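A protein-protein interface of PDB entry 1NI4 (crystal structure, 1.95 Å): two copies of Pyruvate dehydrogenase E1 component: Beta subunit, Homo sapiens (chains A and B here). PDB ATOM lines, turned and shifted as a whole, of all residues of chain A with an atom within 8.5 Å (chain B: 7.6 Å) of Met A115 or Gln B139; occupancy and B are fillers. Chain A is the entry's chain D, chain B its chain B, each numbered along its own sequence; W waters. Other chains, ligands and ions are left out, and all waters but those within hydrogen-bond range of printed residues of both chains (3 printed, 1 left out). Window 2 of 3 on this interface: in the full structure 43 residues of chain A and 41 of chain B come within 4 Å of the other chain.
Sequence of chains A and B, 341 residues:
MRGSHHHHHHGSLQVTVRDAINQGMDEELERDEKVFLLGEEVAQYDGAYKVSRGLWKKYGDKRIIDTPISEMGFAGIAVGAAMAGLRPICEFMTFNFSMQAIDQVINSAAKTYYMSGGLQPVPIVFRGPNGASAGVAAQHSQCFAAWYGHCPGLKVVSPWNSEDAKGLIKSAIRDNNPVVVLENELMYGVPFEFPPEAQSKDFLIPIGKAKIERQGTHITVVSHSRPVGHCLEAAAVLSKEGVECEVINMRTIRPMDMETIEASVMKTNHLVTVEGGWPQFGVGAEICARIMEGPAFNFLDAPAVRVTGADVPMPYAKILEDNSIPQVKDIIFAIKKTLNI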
ATOM      1  N   ASP A 103     -14.772  -4.366   2.023  1.00  0.00           N
ATOM      2  CA  ASP A 103     -15.425  -5.114   0.950  1.00  0.00           C
ATOM      3  C   ASP A 103     -16.060  -4.148  -0.047  1.00  0.00           C
ATOM      4  O   ASP A 103     -15.995  -4.364  -1.256  1.00  0.00           O
ATOM      5  CB  ASP A 103     -16.507  -6.053   1.489  1.00  0.00           C
ATOM      6  CG  ASP A 103     -17.201  -6.834   0.377  1.00  0.00           C
ATOM      7  OD1 ASP A 103     -16.541  -7.690  -0.254  1.00  0.00           O
ATOM      8  OD2 ASP A 103     -18.400  -6.587   0.121  1.00  0.00           O
ATOM      9  N   GLN A 104     -16.678  -3.083   0.462  1.00  0.00           N
ATOM     10  CA  GLN A 104     -17.314  -2.097  -0.408  1.00  0.00           C
ATOM     11  C   GLN A 104     -16.270  -1.379  -1.265  1.00  0.00           C
ATOM     12  O   GLN A 104     -16.515  -1.090  -2.440  1.00  0.00           O
ATOM     13  CB  GLN A 104     -18.104  -1.072   0.423  1.00  0.00           C
ATOM     14  CG  GLN A 104     -19.344  -1.631   1.128  1.00  0.00           C
ATOM     15  CD  GLN A 104     -20.476  -1.980   0.162  1.00  0.00           C
ATOM     16  OE1 GLN A 104     -20.401  -1.691  -1.034  1.00  0.00           O
ATOM     17  NE2 GLN A 104     -21.535  -2.593   0.685  1.00  0.00           N
ATOM     18  N   ILE A 106     -13.165  -2.522  -2.185  1.00  0.00           N
ATOM     19  CA  ILE A 106     -12.599  -3.463  -3.140  1.00  0.00           C
ATOM     20  C   ILE A 106     -13.602  -4.097  -4.104  1.00  0.00           C
ATOM     21  O   ILE A 106     -13.486  -3.935  -5.316  1.00  0.00           O
ATOM     22  CB  ILE A 106     -11.851  -4.598  -2.396  1.00  0.00           C
ATOM     23  CG1 ILE A 106     -10.800  -4.000  -1.457  1.00  0.00           C
ATOM     24  CG2 ILE A 106     -11.198  -5.543  -3.391  1.00  0.00           C
ATOM     25  CD1 ILE A 106      -9.770  -3.137  -2.148  1.00  0.00           C
ATOM     26  N   ASN A 107     -14.589  -4.812  -3.577  1.00  0.00           N
ATOM     27  CA  ASN A 107     -15.551  -5.486  -4.443  1.00  0.00           C
ATOM     28  C   ASN A 107     -16.662  -4.669  -5.088  1.00  0.00           C
ATOM     29  O   ASN A 107     -17.240  -5.104  -6.087  1.00  0.00           O
ATOM     30  CB  ASN A 107     -16.162  -6.680  -3.718  1.00  0.00           C
ATOM     31  CG  ASN A 107     -15.248  -7.891  -3.734  1.00  0.00           C
ATOM     32  OD1 ASN A 107     -14.359  -7.993  -4.579  1.00  0.00           O
ATOM     33  ND2 ASN A 107     -15.474  -8.825  -2.814  1.00  0.00           N
ATOM     34  N   SER A 108     -16.971  -3.499  -4.542  1.00  0.00           N
ATOM     35  CA  SER A 108     -18.022  -2.682  -5.127  1.00  0.00           C
ATOM     36  C   SER A 108     -17.468  -1.486  -5.891  1.00  0.00           C
ATOM     37  O   SER A 108     -17.912  -1.193  -6.990  1.00  0.00           O
ATOM     38  CB  SER A 108     -18.994  -2.195  -4.051  1.00  0.00           C
ATOM     39  OG  SER A 108     -19.714  -3.277  -3.486  1.00  0.00           O
ATOM     40  N   ALA A 109     -16.494  -0.799  -5.318  1.00  0.00           N
ATOM     41  CA  ALA A 109     -15.935   0.373  -5.977  1.00  0.00           C
ATOM     42  C   ALA A 109     -14.896   0.057  -7.045  1.00  0.00           C
ATOM     43  O   ALA A 109     -15.093   0.360  -8.215  1.00  0.00           O
ATOM     44  CB  ALA A 109     -15.328   1.310  -4.938  1.00  0.00           C
ATOM     45  N   ALA A 110     -13.798  -0.569  -6.633  1.00  0.00           N
ATOM     46  CA  ALA A 110     -12.686  -0.878  -7.525  1.00  0.00           C
ATOM     47  C   ALA A 110     -12.885  -1.742  -8.776  1.00  0.00           C
ATOM     48  O   ALA A 110     -12.336  -1.422  -9.833  1.00  0.00           O
ATOM     49  CB  ALA A 110     -11.539  -1.450  -6.709  1.00  0.00           C
ATOM     50  N   LYS A 111     -13.645  -2.827  -8.672  1.00  0.00           N
ATOM     51  CA  LYS A 111     -13.825  -3.732  -9.805  1.00  0.00           C
ATOM     52  C   LYS A 111     -15.008  -3.440 -10.722  1.00  0.00           C
ATOM     53  O   LYS A 111     -15.102  -3.993 -11.818  1.00  0.00           O
ATOM     54  CB  LYS A 111     -13.948  -5.169  -9.290  1.00  0.00           C
ATOM     55  CG  LYS A 111     -12.799  -5.608  -8.396  1.00  0.00           C
ATOM     56  CD  LYS A 111     -13.094  -6.945  -7.725  1.00  0.00           C
ATOM     57  CE  LYS A 111     -11.935  -7.385  -6.839  1.00  0.00           C
ATOM     58  NZ  LYS A 111     -12.223  -8.671  -6.135  1.00  0.00           N
ATOM     59  N   THR A 112     -15.900  -2.569 -10.280  1.00  0.00           N
ATOM     60  CA  THR A 112     -17.096  -2.256 -11.039  1.00  0.00           C
ATOM     61  C   THR A 112     -16.933  -1.762 -12.475  1.00  0.00           C
ATOM     62  O   THR A 112     -17.607  -2.265 -13.370  1.00  0.00           O
ATOM     63  CB  THR A 112     -17.986  -1.292 -10.239  1.00  0.00           C
ATOM     64  OG1 THR A 112     -18.453  -1.978  -9.073  1.00  0.00           O
ATOM     65  CG2 THR A 112     -19.193  -0.848 -11.049  1.00  0.00           C
ATOM     66  N   TYR A 113     -16.054  -0.802 -12.716  1.00  0.00           N
ATOM     67  CA  TYR A 113     -15.888  -0.315 -14.081  1.00  0.00           C
ATOM     68  C   TYR A 113     -15.444  -1.452 -15.005  1.00  0.00           C
ATOM     69  O   TYR A 113     -15.921  -1.571 -16.128  1.00  0.00           O
ATOM     70  CB  TYR A 113     -14.868   0.818 -14.128  1.00  0.00           C
ATOM     71  CG  TYR A 113     -14.861   1.563 -15.440  1.00  0.00           C
ATOM     72  CD1 TYR A 113     -15.998   2.238 -15.883  1.00  0.00           C
ATOM     73  CD2 TYR A 113     -13.718   1.596 -16.244  1.00  0.00           C
ATOM     74  CE1 TYR A 113     -16.001   2.928 -17.093  1.00  0.00           C
ATOM     75  CE2 TYR A 113     -13.710   2.284 -17.457  1.00  0.00           C
ATOM     76  CZ  TYR A 113     -14.856   2.946 -17.869  1.00  0.00           C
ATOM     77  OH  TYR A 113     -14.862   3.631 -19.056  1.00  0.00           O
ATOM     78  N   TYR A 114     -14.535  -2.291 -14.522  1.00  0.00           N
ATOM     79  CA  TYR A 114     -14.032  -3.413 -15.306  1.00  0.00           C
ATOM     80  C   TYR A 114     -15.103  -4.480 -15.533  1.00  0.00           C
ATOM     81  O   TYR A 114     -15.295  -4.952 -16.658  1.00  0.00           O
ATOM     82  CB  TYR A 114     -12.835  -4.049 -14.598  1.00  0.00           C
ATOM     83  CG  TYR A 114     -12.164  -5.145 -15.398  1.00  0.00           C
ATOM     84  CD1 TYR A 114     -11.268  -4.839 -16.421  1.00  0.00           C
ATOM     85  CD2 TYR A 114     -12.426  -6.489 -15.130  1.00  0.00           C
ATOM     86  CE1 TYR A 114     -10.646  -5.842 -17.153  1.00  0.00           C
ATOM     87  CE2 TYR A 114     -11.814  -7.494 -15.854  1.00  0.00           C
ATOM     88  CZ  TYR A 114     -10.922  -7.165 -16.865  1.00  0.00           C
ATOM     89  OH  TYR A 114     -10.306  -8.167 -17.581  1.00  0.00           O
ATOM     90  N   MET A 115     -15.799  -4.856 -14.462  1.00  0.00           N
ATOM     91  CA  MET A 115     -16.838  -5.878 -14.542  1.00  0.00           C
ATOM     92  C   MET A 115     -17.982  -5.504 -15.473  1.00  0.00           C
ATOM     93  O   MET A 115     -18.559  -6.370 -16.127  1.00  0.00           O
ATOM     94  CB  MET A 115     -17.406  -6.188 -13.149  1.00  0.00           C
ATOM     95  CG  MET A 115     -16.415  -6.847 -12.184  1.00  0.00           C
ATOM     96  SD  MET A 115     -17.288  -7.669 -10.632  1.00  0.00           S
ATOM     97  CE  MET A 115     -17.825  -6.054  -9.712  1.00  0.00           C
ATOM     98  N   SER A 116     -18.305  -4.217 -15.532  1.00  0.00           N
ATOM     99  CA  SER A 116     -19.392  -3.739 -16.374  1.00  0.00           C
ATOM    100  C   SER A 116     -18.953  -3.488 -17.814  1.00  0.00           C
ATOM    101  O   SER A 116     -19.749  -3.057 -18.643  1.00  0.00           O
ATOM    102  CB  SER A 116     -19.979  -2.450 -15.795  1.00  0.00           C
ATOM    103  OG  SER A 116     -19.021  -1.409 -15.811  1.00  0.00           O
ATOM    104  N   GLY A 117     -17.685  -3.757 -18.108  1.00  0.00           N
ATOM    105  CA  GLY A 117     -17.185  -3.541 -19.454  1.00  0.00           C
ATOM    106  C   GLY A 117     -17.092  -2.072 -19.823  1.00  0.00           C
ATOM    107  O   GLY A 117     -17.249  -1.708 -20.985  1.00  0.00           O
ATOM    108  N   GLY A 118     -16.850  -1.224 -18.828  1.00  0.00           N
ATOM    109  CA  GLY A 118     -16.729   0.200 -19.080  1.00  0.00           C
ATOM    110  C   GLY A 118     -18.039   0.968 -19.074  1.00  0.00           C
ATOM    111  O   GLY A 118     -18.110   2.061 -19.629  1.00  0.00           O
ATOM    112  N   LEU A 119     -19.072   0.418 -18.448  1.00  0.00           N
ATOM    113  CA  LEU A 119     -20.368   1.093 -18.402  1.00  0.00           C
ATOM    114  C   LEU A 119     -20.648   1.813 -17.084  1.00  0.00           C
ATOM    115  O   LEU A 119     -21.360   2.814 -17.063  1.00  0.00           O
ATOM    116  CB  LEU A 119     -21.499   0.093 -18.674  1.00  0.00           C
ATOM    117  CG  LEU A 119     -22.029  -0.039 -20.111  1.00  0.00           C
ATOM    118  CD1 LEU A 119     -20.891  -0.258 -21.105  1.00  0.00           C
ATOM    119  CD2 LEU A 119     -23.015  -1.201 -20.161  1.00  0.00           C
ATOM    120  N   GLN A 120     -20.091   1.308 -15.986  1.00  0.00           N
ATOM    121  CA  GLN A 120     -20.327   1.912 -14.680  1.00  0.00           C
ATOM    122  C   GLN A 120     -19.082   2.442 -13.970  1.00  0.00           C
ATOM    123  O   GLN A 120     -18.318   1.680 -13.387  1.00  0.00           O
ATOM    124  CB  GLN A 120     -21.027   0.905 -13.764  1.00  0.00           C
ATOM    125  CG  GLN A 120     -21.400   1.468 -12.397  1.00  0.00           C
ATOM    126  CD  GLN A 120     -22.412   2.599 -12.494  1.00  0.00           C
ATOM    127  OE1 GLN A 120     -23.582   2.368 -12.804  1.00  0.00           O
ATOM    128  NE2 GLN A 120     -21.962   3.827 -12.237  1.00  0.00           N
ATOM    129  N   THR B  94     -15.671 -18.851   0.941  1.00  0.00           N
ATOM    130  CA  THR B  94     -14.533 -18.505   0.098  1.00  0.00           C
ATOM    131  C   THR B  94     -13.909 -17.350   0.861  1.00  0.00           C
ATOM    132  O   THR B  94     -14.603 -16.672   1.621  1.00  0.00           O
ATOM    133  CB  THR B  94     -14.928 -18.031  -1.327  1.00  0.00           C
ATOM    134  OG1 THR B  94     -15.488 -16.714  -1.262  1.00  0.00           O
ATOM    135  CG2 THR B  94     -15.924 -18.995  -1.959  1.00  0.00           C
ATOM    136  N   PHE B  95     -12.614 -17.124   0.692  1.00  0.00           N
ATOM    137  CA  PHE B  95     -11.997 -16.034   1.420  1.00  0.00           C
ATOM    138  C   PHE B  95     -12.398 -14.658   0.923  1.00  0.00           C
ATOM    139  O   PHE B  95     -12.126 -13.651   1.583  1.00  0.00           O
ATOM    140  CB  PHE B  95     -10.477 -16.191   1.457  1.00  0.00           C
ATOM    141  CG  PHE B  95     -10.002 -16.947   2.663  1.00  0.00           C
ATOM    142  CD1 PHE B  95      -9.943 -18.336   2.655  1.00  0.00           C
ATOM    143  CD2 PHE B  95      -9.706 -16.271   3.840  1.00  0.00           C
ATOM    144  CE1 PHE B  95      -9.600 -19.042   3.807  1.00  0.00           C
ATOM    145  CE2 PHE B  95      -9.364 -16.963   4.996  1.00  0.00           C
ATOM    146  CZ  PHE B  95      -9.311 -18.354   4.982  1.00  0.00           C
ATOM    147  N   ASN B  96     -13.052 -14.612  -0.235  1.00  0.00           N
ATOM    148  CA  ASN B  96     -13.519 -13.342  -0.760  1.00  0.00           C
ATOM    149  C   ASN B  96     -14.508 -12.799   0.265  1.00  0.00           C
ATOM    150  O   ASN B  96     -14.588 -11.590   0.477  1.00  0.00           O
ATOM    151  CB  ASN B  96     -14.237 -13.533  -2.098  1.00  0.00           C
ATOM    152  CG  ASN B  96     -13.338 -14.115  -3.164  1.00  0.00           C
ATOM    153  OD1 ASN B  96     -12.394 -13.469  -3.616  1.00  0.00           O
ATOM    154  ND2 ASN B  96     -13.625 -15.345  -3.571  1.00  0.00           N
ATOM    155  N   PHE B  97     -15.245 -13.703   0.911  1.00  0.00           N
ATOM    156  CA  PHE B  97     -16.239 -13.303   1.906  1.00  0.00           C
ATOM    157  C   PHE B  97     -15.643 -13.002   3.277  1.00  0.00           C
ATOM    158  O   PHE B  97     -16.366 -12.580   4.179  1.00  0.00           O
ATOM    159  CB  PHE B  97     -17.319 -14.384   2.081  1.00  0.00           C
ATOM    160  CG  PHE B  97     -17.833 -14.964   0.789  1.00  0.00           C
ATOM    161  CD1 PHE B  97     -18.016 -14.160  -0.335  1.00  0.00           C
ATOM    162  CD2 PHE B  97     -18.142 -16.316   0.701  1.00  0.00           C
ATOM    163  CE1 PHE B  97     -18.498 -14.701  -1.533  1.00  0.00           C
ATOM    164  CE2 PHE B  97     -18.628 -16.872  -0.493  1.00  0.00           C
ATOM    165  CZ  PHE B  97     -18.805 -16.063  -1.610  1.00  0.00           C
ATOM    166  N   MET B  99     -13.542 -10.694   3.855  1.00  0.00           N
ATOM    167  CA  MET B  99     -13.291  -9.260   3.940  1.00  0.00           C
ATOM    168  C   MET B  99     -14.263  -8.583   4.892  1.00  0.00           C
ATOM    169  O   MET B  99     -13.898  -7.642   5.597  1.00  0.00           O
ATOM    170  CB  MET B  99     -13.375  -8.603   2.558  1.00  0.00           C
ATOM    171  CG  MET B  99     -12.126  -8.803   1.712  1.00  0.00           C
ATOM    172  SD  MET B  99     -12.015  -7.625   0.161  1.00  0.00           S
ATOM    173  CE  MET B  99     -13.166  -8.626  -1.024  1.00  0.00           C
ATOM    174  N   VAL B 136     -15.736 -17.993 -12.020  1.00  0.00           N
ATOM    175  CA  VAL B 136     -16.473 -17.320 -10.951  1.00  0.00           C
ATOM    176  C   VAL B 136     -16.398 -15.786 -10.978  1.00  0.00           C
ATOM    177  O   VAL B 136     -16.981 -15.122 -10.132  1.00  0.00           O
ATOM    178  CB  VAL B 136     -16.032 -17.830  -9.558  1.00  0.00           C
ATOM    179  CG1 VAL B 136     -16.456 -19.288  -9.386  1.00  0.00           C
ATOM    180  CG2 VAL B 136     -14.523 -17.689  -9.394  1.00  0.00           C
ATOM    181  N   ALA B 137     -15.677 -15.231 -11.944  1.00  0.00           N
ATOM    182  CA  ALA B 137     -15.567 -13.778 -12.093  1.00  0.00           C
ATOM    183  C   ALA B 137     -14.823 -13.024 -10.971  1.00  0.00           C
ATOM    184  O   ALA B 137     -14.434 -13.596  -9.951  1.00  0.00           O
ATOM    185  CB  ALA B 137     -16.961 -13.174 -12.306  1.00  0.00           C
ATOM    186  N   ALA B 138     -14.656 -11.723 -11.189  1.00  0.00           N
ATOM    187  CA  ALA B 138     -13.925 -10.816 -10.309  1.00  0.00           C
ATOM    188  C   ALA B 138     -14.132 -10.827  -8.794  1.00  0.00           C
ATOM    189  O   ALA B 138     -13.153 -10.768  -8.042  1.00  0.00           O
ATOM    190  CB  ALA B 138     -14.091  -9.387 -10.828  1.00  0.00           C
ATOM    191  N   GLN B 139     -15.377 -10.884  -8.333  1.00  0.00           N
ATOM    192  CA  GLN B 139     -15.635 -10.860  -6.897  1.00  0.00           C
ATOM    193  C   GLN B 139     -15.416 -12.190  -6.191  1.00  0.00           C
ATOM    194  O   GLN B 139     -15.471 -12.256  -4.965  1.00  0.00           O
ATOM    195  CB  GLN B 139     -17.065 -10.371  -6.623  1.00  0.00           C
ATOM    196  CG  GLN B 139     -17.408  -9.034  -7.285  1.00  0.00           C
ATOM    197  CD  GLN B 139     -18.737  -8.455  -6.818  1.00  0.00           C
ATOM    198  OE1 GLN B 139     -19.757  -9.148  -6.777  1.00  0.00           O
ATOM    199  NE2 GLN B 139     -18.730  -7.174  -6.471  1.00  0.00           N
ATOM    200  N   HIS B 140     -15.158 -13.247  -6.954  1.00  0.00           N
ATOM    201  CA  HIS B 140     -14.963 -14.568  -6.363  1.00  0.00           C
ATOM    202  C   HIS B 140     -13.615 -15.222  -6.660  1.00  0.00           C
ATOM    203  O   HIS B 140     -13.453 -16.411  -6.416  1.00  0.00           O
ATOM    204  CB  HIS B 140     -16.067 -15.521  -6.839  1.00  0.00           C
ATOM    205  CG  HIS B 140     -17.411 -15.249  -6.239  1.00  0.00           C
ATOM    206  ND1 HIS B 140     -18.121 -14.094  -6.486  1.00  0.00           N
ATOM    207  CD2 HIS B 140     -18.181 -15.992  -5.407  1.00  0.00           C
ATOM    208  CE1 HIS B 140     -19.270 -14.138  -5.836  1.00  0.00           C
ATOM    209  NE2 HIS B 140     -19.331 -15.279  -5.173  1.00  0.00           N
ATOM    210  N   SER B 141     -12.648 -14.459  -7.155  1.00  0.00           N
ATOM    211  CA  SER B 141     -11.358 -15.039  -7.517  1.00  0.00           C
ATOM    212  C   SER B 141     -10.113 -14.441  -6.862  1.00  0.00           C
ATOM    213  O   SER B 141      -8.990 -14.789  -7.238  1.00  0.00           O
ATOM    214  CB  SER B 141     -11.192 -14.960  -9.033  1.00  0.00           C
ATOM    215  OG  SER B 141     -12.359 -15.425  -9.692  1.00  0.00           O
ATOM    216  N   GLN B 142     -10.299 -13.566  -5.880  1.00  0.00           N
ATOM    217  CA  GLN B 142      -9.161 -12.921  -5.230  1.00  0.00           C
ATOM    218  C   GLN B 142      -8.320 -13.822  -4.321  1.00  0.00           C
ATOM    219  O   GLN B 142      -8.857 -14.661  -3.603  1.00  0.00           O
ATOM    220  CB  GLN B 142      -9.648 -11.713  -4.427  1.00  0.00           C
ATOM    221  CG  GLN B 142      -8.555 -10.726  -4.065  1.00  0.00           C
ATOM    222  CD  GLN B 142      -9.104  -9.493  -3.380  1.00  0.00           C
ATOM    223  OE1 GLN B 142     -10.162  -8.985  -3.757  1.00  0.00           O
ATOM    224  NE2 GLN B 142      -8.384  -8.993  -2.377  1.00  0.00           N
ATOM    225  N   PHE B 144      -5.804 -13.981  -1.139  1.00  0.00           N
ATOM    226  CA  PHE B 144      -5.516 -13.157   0.034  1.00  0.00           C
ATOM    227  C   PHE B 144      -4.237 -13.513   0.780  1.00  0.00           C
ATOM    228  O   PHE B 144      -4.051 -13.092   1.919  1.00  0.00           O
ATOM    229  CB  PHE B 144      -6.698 -13.202   1.016  1.00  0.00           C
ATOM    230  CG  PHE B 144      -7.966 -12.609   0.466  1.00  0.00           C
ATOM    231  CD1 PHE B 144      -8.823 -13.370  -0.322  1.00  0.00           C
ATOM    232  CD2 PHE B 144      -8.281 -11.278   0.701  1.00  0.00           C
ATOM    233  CE1 PHE B 144      -9.973 -12.811  -0.868  1.00  0.00           C
ATOM    234  CE2 PHE B 144      -9.430 -10.704   0.159  1.00  0.00           C
ATOM    235  CZ  PHE B 144     -10.277 -11.471  -0.625  1.00  0.00           C
ATOM    236  N   PRO B 313      -8.781  -7.307 -12.505  1.00  0.00           N
ATOM    237  CA  PRO B 313      -9.727  -8.144 -11.769  1.00  0.00           C
ATOM    238  C   PRO B 313     -10.088  -9.306 -12.695  1.00  0.00           C
ATOM    239  O   PRO B 313     -10.096  -9.155 -13.916  1.00  0.00           O
ATOM    240  CB  PRO B 313     -10.885  -7.192 -11.474  1.00  0.00           C
ATOM    241  CG  PRO B 313     -10.790  -6.173 -12.546  1.00  0.00           C
ATOM    242  CD  PRO B 313      -9.321  -5.959 -12.745  1.00  0.00           C
ATOM    243  N   MET B 314     -10.360 -10.467 -12.112  1.00  0.00           N
ATOM    244  CA  MET B 314     -10.658 -11.667 -12.890  1.00  0.00           C
ATOM    245  C   MET B 314     -11.821 -11.573 -13.883  1.00  0.00           C
ATOM    246  O   MET B 314     -12.969 -11.340 -13.501  1.00  0.00           O
ATOM    247  CB  MET B 314     -10.891 -12.851 -11.945  1.00  0.00           C
ATOM    248  CG  MET B 314     -10.902 -14.207 -12.638  1.00  0.00           C
ATOM    249  SD  MET B 314      -9.164 -14.666 -13.389  1.00  0.00           S
ATOM    250  CE  MET B 314      -8.252 -15.130 -11.737  1.00  0.00           C
ATOM    251  N   PRO B 315     -11.528 -11.748 -15.179  1.00  0.00           N
ATOM    252  CA  PRO B 315     -12.580 -11.686 -16.201  1.00  0.00           C
ATOM    253  C   PRO B 315     -13.340 -13.014 -16.228  1.00  0.00           C
ATOM    254  O   PRO B 315     -12.870 -14.019 -15.686  1.00  0.00           O
ATOM    255  CB  PRO B 315     -11.796 -11.435 -17.479  1.00  0.00           C
ATOM    256  CG  PRO B 315     -10.509 -12.190 -17.218  1.00  0.00           C
ATOM    257  CD  PRO B 315     -10.191 -11.807 -15.800  1.00  0.00           C
HETATM  258  O   HOH W   1     -15.779  -5.288   4.651  1.00  0.00           O
HETATM  259  O   HOH W   2     -21.073  -4.912  -5.759  1.00  0.00           O
HETATM  260  O   HOH W   3     -16.469  -9.841   1.672  1.00  0.00           O
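O of Ala B138 lies within hydrogen-bond range of NZ of Lys A111 (3.0 Å). O of Asn A107 sits at hydrogen-bond distance from NE2 of Gln B139, at 2.6 Å. OE1 of Gln B142 lies within hydrogen-bond range of NZ of Lys A111, 3.2 Å away.
The backbone NH (N) of Gln B142 is in hydrogen-bond range of the side-chain amide oxygen (OD1) of Asn B96, 3.1 Å away. N of Ala B138 is in hydrogen-bond range of O of Met B314, 2.9 Å away. ND2 of Asn A107 lies within hydrogen-bond range of OD1 of Asp A103, 3.0 Å away. The side-chain amide oxygen of Asn A107 sits at hydrogen-bond distance from the side-chain amino group of Lys A111, 2.7 Å away.
Among the printed residues, pairs that only touch across the chains: Asp A103 with Met B99, Ile A106 with Met B99, Ile A106 with Gln B142, Asn A107 with Met B99, Lys A111 with Pro B313, Tyr A114 with Pro B313, Tyr A114 with Pro B315, Met A115 with Ala B138 and Met A115 with Gln B139.
Of the printed residues of chain B, Asp A103 touches Met B99 (3.6 Å). Thr A112 touches none of the printed residues of chain B. Of the printed residues of chain B, Met A115 touches Ala B138 and Gln B139. Ala B138 touches two residues of chain A. Gln B139 touches two residues of chain A. Of the printed residues of chain A, Pro B313 touches Lys A111 (3.96 Å) and Tyr A114 (3.1 Å). The nearest printed residue of chain B that does not touch Lys A111 is Gln B139 (4.1 Å).
Printed residues of chain B that touch a printed residue of chain A: Met B99, Ala B138, Gln B139, Gln B142, Pro B313 and Pro B315. Hydrophobic or aromatic side chains of chain B within 4 Å of the printed part of chain A: Met B99, Ala B138, Pro B313 and Pro B315. Among the printed residues, 12 pairs touch across the chains.
No position is printed for both chains. Of the 12 pairs that touch across the chains among the printed residues, none has its exchanged pair printed and touching as well.
Water W3 bridges O of Asn B96 (2.8 Å) and OD1 of Asp A103 (2.9 Å). Water W1 lies within hydrogen-bond range of N of Asp A103 and O of Met B99. Water W2 bridges the side-chain hydroxyl of Ser A108 (3.1 Å) and the side-chain amide nitrogen of Gln B139 (3.3 Å).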
